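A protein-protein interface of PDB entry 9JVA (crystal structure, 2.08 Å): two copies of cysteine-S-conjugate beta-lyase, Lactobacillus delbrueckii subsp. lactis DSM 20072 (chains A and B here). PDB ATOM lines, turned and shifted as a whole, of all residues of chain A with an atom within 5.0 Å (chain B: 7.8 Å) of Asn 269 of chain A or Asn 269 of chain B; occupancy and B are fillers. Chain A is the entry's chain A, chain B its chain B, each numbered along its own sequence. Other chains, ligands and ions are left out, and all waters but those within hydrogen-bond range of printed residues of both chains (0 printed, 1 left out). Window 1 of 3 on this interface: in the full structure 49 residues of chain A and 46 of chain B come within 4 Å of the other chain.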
ATOM      1  N   GLU A  60      -3.924  17.851 -15.668  1.00  0.00           N
ATOM      2  CA  GLU A  60      -2.790  18.661 -15.242  1.00  0.00           C
ATOM      3  C   GLU A  60      -3.117  20.140 -15.329  1.00  0.00           C
ATOM      4  O   GLU A  60      -3.734  20.592 -16.296  1.00  0.00           O
ATOM      5  CB  GLU A  60      -1.566  18.372 -16.112  1.00  0.00           C
ATOM      6  CG  GLU A  60      -1.036  16.988 -15.915  1.00  0.00           C
ATOM      7  CD  GLU A  60       0.260  16.778 -16.634  1.00  0.00           C
ATOM      8  OE1 GLU A  60       0.516  15.629 -17.060  1.00  0.00           O
ATOM      9  OE2 GLU A  60       1.009  17.773 -16.763  1.00  0.00           O
ATOM     10  N   ALA A 239       5.910  17.993 -32.140  1.00  0.00           N
ATOM     11  CA  ALA A 239       4.833  17.134 -31.663  1.00  0.00           C
ATOM     12  C   ALA A 239       4.614  17.232 -30.154  1.00  0.00           C
ATOM     13  O   ALA A 239       3.759  16.520 -29.629  1.00  0.00           O
ATOM     14  CB  ALA A 239       5.097  15.675 -32.070  1.00  0.00           C
ATOM     15  N   LEU A 240       5.355  18.102 -29.449  1.00  0.00           N
ATOM     16  CA  LEU A 240       5.160  18.248 -28.007  1.00  0.00           C
ATOM     17  C   LEU A 240       3.886  19.019 -27.684  1.00  0.00           C
ATOM     18  O   LEU A 240       3.271  18.772 -26.640  1.00  0.00           O
ATOM     19  CB  LEU A 240       6.363  18.944 -27.357  1.00  0.00           C
ATOM     20  CG  LEU A 240       6.263  19.182 -25.839  1.00  0.00           C
ATOM     21  CD1 LEU A 240       6.195  17.853 -25.080  1.00  0.00           C
ATOM     22  CD2 LEU A 240       7.394  20.061 -25.294  1.00  0.00           C
ATOM     23  N   HIS A 241       3.494  19.961 -28.546  1.00  0.00           N
ATOM     24  CA  HIS A 241       2.263  20.749 -28.368  1.00  0.00           C
ATOM     25  C   HIS A 241       2.327  21.585 -27.086  1.00  0.00           C
ATOM     26  O   HIS A 241       1.425  21.548 -26.249  1.00  0.00           O
ATOM     27  CB  HIS A 241       1.006  19.865 -28.367  1.00  0.00           C
ATOM     28  CG  HIS A 241       0.698  19.207 -29.677  1.00  0.00           C
ATOM     29  ND1 HIS A 241       1.508  19.312 -30.786  1.00  0.00           N
ATOM     30  CD2 HIS A 241      -0.328  18.403 -30.042  1.00  0.00           C
ATOM     31  CE1 HIS A 241       0.993  18.614 -31.781  1.00  0.00           C
ATOM     32  NE2 HIS A 241      -0.122  18.051 -31.356  1.00  0.00           N
ATOM     33  N   GLU A 267      -5.065  23.368 -22.438  1.00  0.00           N
ATOM     34  CA  GLU A 267      -4.676  22.439 -21.388  1.00  0.00           C
ATOM     35  C   GLU A 267      -3.540  21.541 -21.857  1.00  0.00           C
ATOM     36  O   GLU A 267      -3.584  21.021 -22.986  1.00  0.00           O
ATOM     37  CB  GLU A 267      -5.878  21.592 -20.939  1.00  0.00           C
ATOM     38  CG  GLU A 267      -7.027  22.465 -20.442  1.00  0.00           C
ATOM     39  CD  GLU A 267      -8.031  21.732 -19.573  1.00  0.00           C
ATOM     40  OE1 GLU A 267      -7.792  20.554 -19.220  1.00  0.00           O
ATOM     41  OE2 GLU A 267      -9.059  22.355 -19.230  1.00  0.00           O
ATOM     42  N   PRO A 268      -2.510  21.342 -21.037  1.00  0.00           N
ATOM     43  CA  PRO A 268      -1.325  20.606 -21.490  1.00  0.00           C
ATOM     44  C   PRO A 268      -1.567  19.107 -21.553  1.00  0.00           C
ATOM     45  O   PRO A 268      -2.312  18.528 -20.756  1.00  0.00           O
ATOM     46  CB  PRO A 268      -0.277  20.945 -20.423  1.00  0.00           C
ATOM     47  CG  PRO A 268      -1.091  21.263 -19.184  1.00  0.00           C
ATOM     48  CD  PRO A 268      -2.341  21.920 -19.690  1.00  0.00           C
ATOM     49  N   ASN A 269      -0.918  18.480 -22.528  1.00  0.00           N
ATOM     50  CA  ASN A 269      -0.844  17.035 -22.541  1.00  0.00           C
ATOM     51  C   ASN A 269       0.173  16.581 -21.492  1.00  0.00           C
ATOM     52  O   ASN A 269       0.775  17.388 -20.777  1.00  0.00           O
ATOM     53  CB  ASN A 269      -0.509  16.520 -23.944  1.00  0.00           C
ATOM     54  CG  ASN A 269       0.884  16.921 -24.413  1.00  0.00           C
ATOM     55  OD1 ASN A 269       1.860  16.773 -23.685  1.00  0.00           O
ATOM     56  ND2 ASN A 269       0.984  17.391 -25.660  1.00  0.00           N
ATOM     57  N   LEU A 270       0.409  15.270 -21.440  1.00  0.00           N
ATOM     58  CA  LEU A 270       1.160  14.667 -20.346  1.00  0.00           C
ATOM     59  C   LEU A 270       2.646  15.040 -20.334  1.00  0.00           C
ATOM     60  O   LEU A 270       3.302  14.851 -19.307  1.00  0.00           O
ATOM     61  CB  LEU A 270       0.984  13.148 -20.401  1.00  0.00           C
ATOM     62  CG  LEU A 270       1.718  12.271 -21.431  1.00  0.00           C
ATOM     63  CD1 LEU A 270       1.191  10.861 -21.304  1.00  0.00           C
ATOM     64  CD2 LEU A 270       1.582  12.718 -22.902  1.00  0.00           C
ATOM     65  N   LEU A 271       3.199  15.550 -21.436  1.00  0.00           N
ATOM     66  CA  LEU A 271       4.613  15.898 -21.477  1.00  0.00           C
ATOM     67  C   LEU A 271       4.873  17.390 -21.614  1.00  0.00           C
ATOM     68  O   LEU A 271       5.997  17.829 -21.339  1.00  0.00           O
ATOM     69  CB  LEU A 271       5.316  15.153 -22.625  1.00  0.00           C
ATOM     70  CG  LEU A 271       5.484  13.642 -22.398  1.00  0.00           C
ATOM     71  CD1 LEU A 271       6.273  12.996 -23.546  1.00  0.00           C
ATOM     72  CD2 LEU A 271       6.124  13.343 -21.036  1.00  0.00           C
ATOM     73  N   ALA A 272       3.864  18.177 -22.008  1.00  0.00           N
ATOM     74  CA  ALA A 272       4.091  19.573 -22.382  1.00  0.00           C
ATOM     75  C   ALA A 272       4.771  20.360 -21.262  1.00  0.00           C
ATOM     76  O   ALA A 272       5.725  21.110 -21.510  1.00  0.00           O
ATOM     77  CB  ALA A 272       2.771  20.236 -22.773  1.00  0.00           C
ATOM     78  N   ILE A 273       4.299  20.209 -20.026  1.00  0.00           N
ATOM     79  CA  ILE A 273       4.795  21.038 -18.924  1.00  0.00           C
ATOM     80  C   ILE A 273       6.233  20.664 -18.563  1.00  0.00           C
ATOM     81  O   ILE A 273       7.109  21.531 -18.687  1.00  0.00           O
ATOM     82  CB  ILE A 273       3.874  20.977 -17.688  1.00  0.00           C
ATOM     83  CG1 ILE A 273       2.475  21.526 -18.017  1.00  0.00           C
ATOM     84  CG2 ILE A 273       4.493  21.785 -16.550  1.00  0.00           C
ATOM     85  CD1 ILE A 273       2.500  22.881 -18.723  1.00  0.00           C
ATOM     86  N   ASN B  17       1.738  19.390 -10.484  1.00  0.00           N
ATOM     87  CA  ASN B  17       0.650  20.076 -11.171  1.00  0.00           C
ATOM     88  C   ASN B  17      -0.543  19.163 -11.442  1.00  0.00           C
ATOM     89  O   ASN B  17      -1.372  19.476 -12.301  1.00  0.00           O
ATOM     90  CB  ASN B  17       1.159  20.707 -12.474  1.00  0.00           C
ATOM     91  CG  ASN B  17       1.613  19.671 -13.488  1.00  0.00           C
ATOM     92  OD1 ASN B  17       2.230  18.675 -13.130  1.00  0.00           O
ATOM     93  ND2 ASN B  17       1.324  19.911 -14.758  1.00  0.00           N
ATOM     94  N   LYS B  51       8.604   4.893 -27.874  1.00  0.00           N
ATOM     95  CA  LYS B  51       8.510   6.085 -28.710  1.00  0.00           C
ATOM     96  C   LYS B  51       9.542   7.126 -28.304  1.00  0.00           C
ATOM     97  O   LYS B  51      10.110   7.815 -29.160  1.00  0.00           O
ATOM     98  CB  LYS B  51       7.099   6.670 -28.627  1.00  0.00           C
ATOM     99  CG  LYS B  51       6.887   7.977 -29.417  1.00  0.00           C
ATOM    100  CD  LYS B  51       7.245   7.826 -30.907  1.00  0.00           C
ATOM    101  CE  LYS B  51       7.040   9.134 -31.659  1.00  0.00           C
ATOM    102  NZ  LYS B  51       5.583   9.405 -31.834  1.00  0.00           N
ATOM    103  N   PHE B  57      11.107  14.816 -32.016  1.00  0.00           N
ATOM    104  CA  PHE B  57       9.658  14.754 -32.035  1.00  0.00           C
ATOM    105  C   PHE B  57       9.090  15.801 -32.986  1.00  0.00           C
ATOM    106  O   PHE B  57       8.462  16.782 -32.591  1.00  0.00           O
ATOM    107  CB  PHE B  57       9.113  14.879 -30.614  1.00  0.00           C
ATOM    108  CG  PHE B  57       9.695  13.849 -29.697  1.00  0.00           C
ATOM    109  CD1 PHE B  57       9.340  12.511 -29.842  1.00  0.00           C
ATOM    110  CD2 PHE B  57      10.667  14.196 -28.765  1.00  0.00           C
ATOM    111  CE1 PHE B  57       9.921  11.527 -29.036  1.00  0.00           C
ATOM    112  CE2 PHE B  57      11.245  13.220 -27.949  1.00  0.00           C
ATOM    113  CZ  PHE B  57      10.865  11.886 -28.091  1.00  0.00           C
ATOM    114  N   GLY B  58       9.304  15.559 -34.276  1.00  0.00           N
ATOM    115  CA  GLY B  58       8.736  16.389 -35.316  1.00  0.00           C
ATOM    116  C   GLY B  58       7.306  15.985 -35.634  1.00  0.00           C
ATOM    117  O   GLY B  58       6.656  15.229 -34.910  1.00  0.00           O
ATOM    118  N   GLU B  60       3.829  14.541 -36.955  1.00  0.00           N
ATOM    119  CA  GLU B  60       3.345  13.185 -37.127  1.00  0.00           C
ATOM    120  C   GLU B  60       2.057  13.138 -37.939  1.00  0.00           C
ATOM    121  O   GLU B  60       1.215  14.044 -37.872  1.00  0.00           O
ATOM    122  CB  GLU B  60       3.121  12.525 -35.771  1.00  0.00           C
ATOM    123  CG  GLU B  60       4.413  12.069 -35.157  1.00  0.00           C
ATOM    124  CD  GLU B  60       4.193  11.315 -33.881  1.00  0.00           C
ATOM    125  OE1 GLU B  60       4.987  11.514 -32.941  1.00  0.00           O
ATOM    126  OE2 GLU B  60       3.208  10.538 -33.816  1.00  0.00           O
ATOM    127  N   SER B  61       1.912  12.052 -38.692  1.00  0.00           N
ATOM    128  CA  SER B  61       0.685  11.697 -39.386  1.00  0.00           C
ATOM    129  C   SER B  61      -0.074  10.642 -38.578  1.00  0.00           C
ATOM    130  O   SER B  61       0.449  10.049 -37.626  1.00  0.00           O
ATOM    131  CB  SER B  61       1.006  11.178 -40.790  1.00  0.00           C
ATOM    132  OG  SER B  61       1.736   9.969 -40.710  1.00  0.00           O
ATOM    133  N   PHE B  89      -8.863  10.926 -36.326  1.00  0.00           N
ATOM    134  CA  PHE B  89      -8.192  11.300 -35.083  1.00  0.00           C
ATOM    135  C   PHE B  89      -8.577  12.714 -34.625  1.00  0.00           C
ATOM    136  O   PHE B  89      -8.684  13.644 -35.427  1.00  0.00           O
ATOM    137  CB  PHE B  89      -6.675  11.211 -35.269  1.00  0.00           C
ATOM    138  CG  PHE B  89      -5.905  11.681 -34.076  1.00  0.00           C
ATOM    139  CD1 PHE B  89      -5.561  13.013 -33.939  1.00  0.00           C
ATOM    140  CD2 PHE B  89      -5.552  10.785 -33.079  1.00  0.00           C
ATOM    141  CE1 PHE B  89      -4.871  13.457 -32.822  1.00  0.00           C
ATOM    142  CE2 PHE B  89      -4.870  11.218 -31.951  1.00  0.00           C
ATOM    143  CZ  PHE B  89      -4.522  12.551 -31.827  1.00  0.00           C
ATOM    144  N   SER B  91      -7.540  15.322 -30.993  1.00  0.00           N
ATOM    145  CA  SER B  91      -6.771  15.432 -29.754  1.00  0.00           C
ATOM    146  C   SER B  91      -7.610  15.265 -28.490  1.00  0.00           C
ATOM    147  O   SER B  91      -7.044  15.115 -27.402  1.00  0.00           O
ATOM    148  CB  SER B  91      -6.058  16.776 -29.727  1.00  0.00           C
ATOM    149  OG  SER B  91      -5.005  16.733 -30.680  1.00  0.00           O
ATOM    150  N   ALA B 238      -6.152  10.746 -19.485  1.00  0.00           N
ATOM    151  CA  ALA B 238      -6.774  12.041 -19.825  1.00  0.00           C
ATOM    152  C   ALA B 238      -5.773  13.006 -20.496  1.00  0.00           C
ATOM    153  O   ALA B 238      -6.171  13.696 -21.423  1.00  0.00           O
ATOM    154  CB  ALA B 238      -7.355  12.657 -18.594  1.00  0.00           C
ATOM    155  N   ALA B 239      -4.542  13.059 -19.997  1.00  0.00           N
ATOM    156  CA  ALA B 239      -3.582  13.992 -20.580  1.00  0.00           C
ATOM    157  C   ALA B 239      -2.857  13.437 -21.801  1.00  0.00           C
ATOM    158  O   ALA B 239      -1.947  14.099 -22.316  1.00  0.00           O
ATOM    159  CB  ALA B 239      -2.547  14.424 -19.535  1.00  0.00           C
ATOM    160  N   LEU B 240      -3.220  12.245 -22.281  1.00  0.00           N
ATOM    161  CA  LEU B 240      -2.610  11.756 -23.516  1.00  0.00           C
ATOM    162  C   LEU B 240      -3.086  12.553 -24.723  1.00  0.00           C
ATOM    163  O   LEU B 240      -2.334  12.717 -25.695  1.00  0.00           O
ATOM    164  CB  LEU B 240      -2.922  10.278 -23.720  1.00  0.00           C
ATOM    165  CG  LEU B 240      -2.337   9.634 -24.983  1.00  0.00           C
ATOM    166  CD1 LEU B 240      -0.814   9.640 -24.953  1.00  0.00           C
ATOM    167  CD2 LEU B 240      -2.885   8.216 -25.186  1.00  0.00           C
ATOM    168  N   HIS B 241      -4.328  13.039 -24.676  1.00  0.00           N
ATOM    169  CA  HIS B 241      -4.947  13.794 -25.765  1.00  0.00           C
ATOM    170  C   HIS B 241      -4.999  12.966 -27.050  1.00  0.00           C
ATOM    171  O   HIS B 241      -4.523  13.373 -28.113  1.00  0.00           O
ATOM    172  CB  HIS B 241      -4.244  15.136 -25.982  1.00  0.00           C
ATOM    173  CG  HIS B 241      -4.412  16.090 -24.839  1.00  0.00           C
ATOM    174  ND1 HIS B 241      -3.949  17.388 -24.878  1.00  0.00           N
ATOM    175  CD2 HIS B 241      -4.985  15.933 -23.621  1.00  0.00           C
ATOM    176  CE1 HIS B 241      -4.229  17.988 -23.731  1.00  0.00           C
ATOM    177  NE2 HIS B 241      -4.857  17.126 -22.952  1.00  0.00           N
ATOM    178  N   ALA B 242      -5.593  11.780 -26.943  1.00  0.00           N
ATOM    179  CA  ALA B 242      -5.840  10.927 -28.099  1.00  0.00           C
ATOM    180  C   ALA B 242      -7.319  10.566 -28.102  1.00  0.00           C
ATOM    181  O   ALA B 242      -7.845  10.103 -27.089  1.00  0.00           O
ATOM    182  CB  ALA B 242      -4.968   9.666 -28.070  1.00  0.00           C
ATOM    183  N   GLY B 266      -6.256  18.370 -34.759  1.00  0.00           N
ATOM    184  CA  GLY B 266      -6.299  17.299 -35.737  1.00  0.00           C
ATOM    185  C   GLY B 266      -5.005  16.509 -35.839  1.00  0.00           C
ATOM    186  O   GLY B 266      -4.970  15.452 -36.476  1.00  0.00           O
ATOM    187  N   GLU B 267      -3.939  17.004 -35.209  1.00  0.00           N
ATOM    188  CA  GLU B 267      -2.603  16.419 -35.313  1.00  0.00           C
ATOM    189  C   GLU B 267      -2.188  15.767 -33.998  1.00  0.00           C
ATOM    190  O   GLU B 267      -2.290  16.407 -32.941  1.00  0.00           O
ATOM    191  CB  GLU B 267      -1.594  17.504 -35.695  1.00  0.00           C
ATOM    192  CG  GLU B 267      -0.144  17.069 -35.623  1.00  0.00           C
ATOM    193  CD  GLU B 267       0.828  18.252 -35.733  1.00  0.00           C
ATOM    194  OE1 GLU B 267       1.535  18.556 -34.728  1.00  0.00           O
ATOM    195  OE2 GLU B 267       0.886  18.865 -36.829  1.00  0.00           O
ATOM    196  N   PRO B 268      -1.710  14.522 -34.004  1.00  0.00           N
ATOM    197  CA  PRO B 268      -1.329  13.882 -32.734  1.00  0.00           C
ATOM    198  C   PRO B 268      -0.068  14.485 -32.140  1.00  0.00           C
ATOM    199  O   PRO B 268       0.852  14.906 -32.849  1.00  0.00           O
ATOM    200  CB  PRO B 268      -1.110  12.415 -33.121  1.00  0.00           C
ATOM    201  CG  PRO B 268      -0.817  12.456 -34.580  1.00  0.00           C
ATOM    202  CD  PRO B 268      -1.626  13.590 -35.141  1.00  0.00           C
ATOM    203  N   ASN B 269      -0.026  14.506 -30.812  1.00  0.00           N
ATOM    204  CA  ASN B 269       1.225  14.794 -30.129  1.00  0.00           C
ATOM    205  C   ASN B 269       2.134  13.565 -30.178  1.00  0.00           C
ATOM    206  O   ASN B 269       1.760  12.501 -30.681  1.00  0.00           O
ATOM    207  CB  ASN B 269       0.975  15.248 -28.690  1.00  0.00           C
ATOM    208  CG  ASN B 269       0.362  14.163 -27.821  1.00  0.00           C
ATOM    209  OD1 ASN B 269       0.873  13.044 -27.733  1.00  0.00           O
ATOM    210  ND2 ASN B 269      -0.741  14.504 -27.144  1.00  0.00           N
ATOM    211  N   LEU B 270       3.329  13.707 -29.601  1.00  0.00           N
ATOM    212  CA  LEU B 270       4.396  12.720 -29.755  1.00  0.00           C
ATOM    213  C   LEU B 270       4.061  11.346 -29.163  1.00  0.00           C
ATOM    214  O   LEU B 270       4.729  10.370 -29.501  1.00  0.00           O
ATOM    215  CB  LEU B 270       5.692  13.279 -29.139  1.00  0.00           C
ATOM    216  CG  LEU B 270       5.885  13.433 -27.612  1.00  0.00           C
ATOM    217  CD1 LEU B 270       7.175  14.152 -27.291  1.00  0.00           C
ATOM    218  CD2 LEU B 270       4.741  14.175 -26.912  1.00  0.00           C
ATOM    219  N   LEU B 271       3.065  11.230 -28.285  1.00  0.00           N
ATOM    220  CA  LEU B 271       2.751   9.936 -27.692  1.00  0.00           C
ATOM    221  C   LEU B 271       1.393   9.380 -28.096  1.00  0.00           C
ATOM    222  O   LEU B 271       1.169   8.175 -27.945  1.00  0.00           O
ATOM    223  CB  LEU B 271       2.815  10.026 -26.157  1.00  0.00           C
ATOM    224  CG  LEU B 271       4.228  10.101 -25.560  1.00  0.00           C
ATOM    225  CD1 LEU B 271       4.149   9.983 -24.038  1.00  0.00           C
ATOM    226  CD2 LEU B 271       5.149   9.018 -26.144  1.00  0.00           C
ATOM    227  N   ALA B 272       0.489  10.225 -28.605  1.00  0.00           N
ATOM    228  CA  ALA B 272      -0.909   9.829 -28.757  1.00  0.00           C
ATOM    229  C   ALA B 272      -1.061   8.574 -29.617  1.00  0.00           C
ATOM    230  O   ALA B 272      -1.842   7.676 -29.285  1.00  0.00           O
ATOM    231  CB  ALA B 272      -1.706  10.992 -29.352  1.00  0.00           C
ATOM    232  N   ILE B 273      -0.324   8.481 -30.716  1.00  0.00           N
ATOM    233  CA  ILE B 273      -0.525   7.364 -31.638  1.00  0.00           C
ATOM    234  C   ILE B 273       0.008   6.050 -31.075  1.00  0.00           C
ATOM    235  O   ILE B 273      -0.761   5.082 -31.005  1.00  0.00           O
ATOM    236  CB  ILE B 273       0.088   7.646 -33.019  1.00  0.00           C
ATOM    237  CG1 ILE B 273      -0.586   8.862 -33.673  1.00  0.00           C
ATOM    238  CG2 ILE B 273      -0.017   6.386 -33.885  1.00  0.00           C
ATOM    239  CD1 ILE B 273      -2.128   8.786 -33.710  1.00  0.00           C
ATOM    240  N   PRO B 274       1.289   5.931 -30.684  1.00  0.00           N
ATOM    241  CA  PRO B 274       1.728   4.630 -30.147  1.00  0.00           C
ATOM    242  C   PRO B 274       0.998   4.221 -28.869  1.00  0.00           C
ATOM    243  O   PRO B 274       0.689   3.032 -28.701  1.00  0.00           O
ATOM    244  CB  PRO B 274       3.239   4.826 -29.933  1.00  0.00           C
ATOM    245  CG  PRO B 274       3.425   6.298 -29.826  1.00  0.00           C
ATOM    246  CD  PRO B 274       2.395   6.908 -30.722  1.00  0.00           C
ATOM    247  N   ALA B 275       0.677   5.175 -27.985  1.00  0.00           N
ATOM    248  CA  ALA B 275      -0.009   4.835 -26.740  1.00  0.00           C
ATOM    249  C   ALA B 275      -1.436   4.348 -26.992  1.00  0.00           C
ATOM    250  O   ALA B 275      -1.864   3.337 -26.417  1.00  0.00           O
ATOM    251  CB  ALA B 275      -0.006   6.036 -25.795  1.00  0.00           C
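The backbone carbonyl oxygen (O) of Ala 239 of chain B sits at hydrogen-bond distance from the backbone NH (N) of Leu 270 of chain A, at 2.8 Å. The side-chain carboxylate (OE2) of Glu 60 of chain A lies within hydrogen-bond range of the side-chain amide nitrogen (ND2) of Asn 17 of chain B (2.9 Å). NE2 of His 241 of chain A sits at hydrogen-bond distance from O of Glu 267 of chain B. O of Ala 239 of chain A lies within hydrogen-bond range of N of Leu 270 of chain B. N of Ala 239 of chain A lies within hydrogen-bond range of O of Phe 57 of chain B.
The side-chain amide nitrogen (ND2) of Asn 269 of chain B is in hydrogen-bond range of the backbone carbonyl oxygen (O) of Leu 240 of chain B (2.8 Å). OD1 of Asn 269 of chain A is in hydrogen-bond range of N of Leu 271 of chain A (2.9 Å). The backbone NH (N) of Ala 272 of chain B lies within hydrogen-bond range of the side-chain amide oxygen (OD1) of Asn 269 of chain B, 3.0 Å away. The side-chain amide oxygen (OD1) of Asn 269 of chain B is in hydrogen-bond range of the backbone NH (N) of Leu 271 of chain B. The backbone NH (N) of Ala 272 of chain A sits at hydrogen-bond distance from the side-chain amide oxygen (OD1) of Asn 269 of chain A (3.0 Å). The backbone carbonyl oxygen of Leu 240 of chain A is in hydrogen-bond range of the side-chain amide nitrogen of Asn 269 of chain A (2.8 Å).
Among the printed residues, pairs that only touch across the chains: Ala 239 of chain A with Gly 58 of chain B, Ala 239 of chain A with Asn 269 of chain B, His 241 of chain A with Pro 268 of chain B, His 241 of chain A with Asn 269 of chain B, Glu 267 of chain A with His 241 of chain B, Pro 268 of chain A with His 241 of chain B, Asn 269 of chain A with Ala 239 of chain B, Asn 269 of chain A with His 241 of chain B, Asn 269 of chain A with Asn 269 of chain B, Leu 270 of chain A with Leu 271 of chain B, Leu 271 of chain A with Leu 270 of chain B, Leu 271 of chain A with Leu 271 of chain B and Ile 273 of chain A with Asn 17 of chain B.
Of the printed residues of chain B, Ala 239 of chain A touches Phe 57, Gly 58, Asn 269 and Leu 270. Printed residues of chain B within 4 Å of Glu 267 of chain A: His 241. Printed residues of chain B within 4 Å of Ile 273 of chain A: Asn 17 (3.8 Å). Glu 60 of chain B touches none of the printed residues of chain A. Of the printed residues of chain A, His 241 of chain B touches Glu 267 (3.2 Å), Pro 268 (3.6 Å) and Asn 269 (3.6 Å). The nearest residue of chain B that does not touch Asn 269 of chain A is Leu 240 of chain B (4.6 Å). The nearest printed residue of chain B that does not touch Leu 270 of chain A is Leu 240 of chain B (4.3 Å).
Printed residues of chain B that touch a printed residue of chain A: Asn 17, Phe 57, Gly 58, Ala 239, His 241, Glu 267, Pro 268, Asn 269, Leu 270 and Leu 271. Hydrophobic or aromatic side chains of chain B within 4 Å of the printed part of chain A: Ala 239, His 241, Leu 270 and Leu 271. Along chain B the printed residues that touch a printed residue of chain A span positions 17 to 271. Among the printed residues, 18 pairs touch across the chains. Among the printed residues, no Asp or Glu carboxylate lies within 4 Å of a Lys or Arg side-chain nitrogen of the other chain.
Ala 239 of chain A touches Asn 269 of chain B, and with the chains exchanged Asn 269 of chain A touches Ala 239 of chain B. Ala 239 of chain A touches Leu 270 of chain B, and with the chains exchanged Leu 270 of chain A touches Ala 239 of chain B. His 241 of chain A touches Pro 268 of chain B, and with the chains exchanged Pro 268 of chain A touches His 241 of chain B. His 241 of chain A touches Asn 269 of chain B, and with the chains exchanged Asn 269 of chain A touches His 241 of chain B. Positions printed for both chains: 60, 239, 240, 241, 267, 268, 269, 270, 271, 272 and 273.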
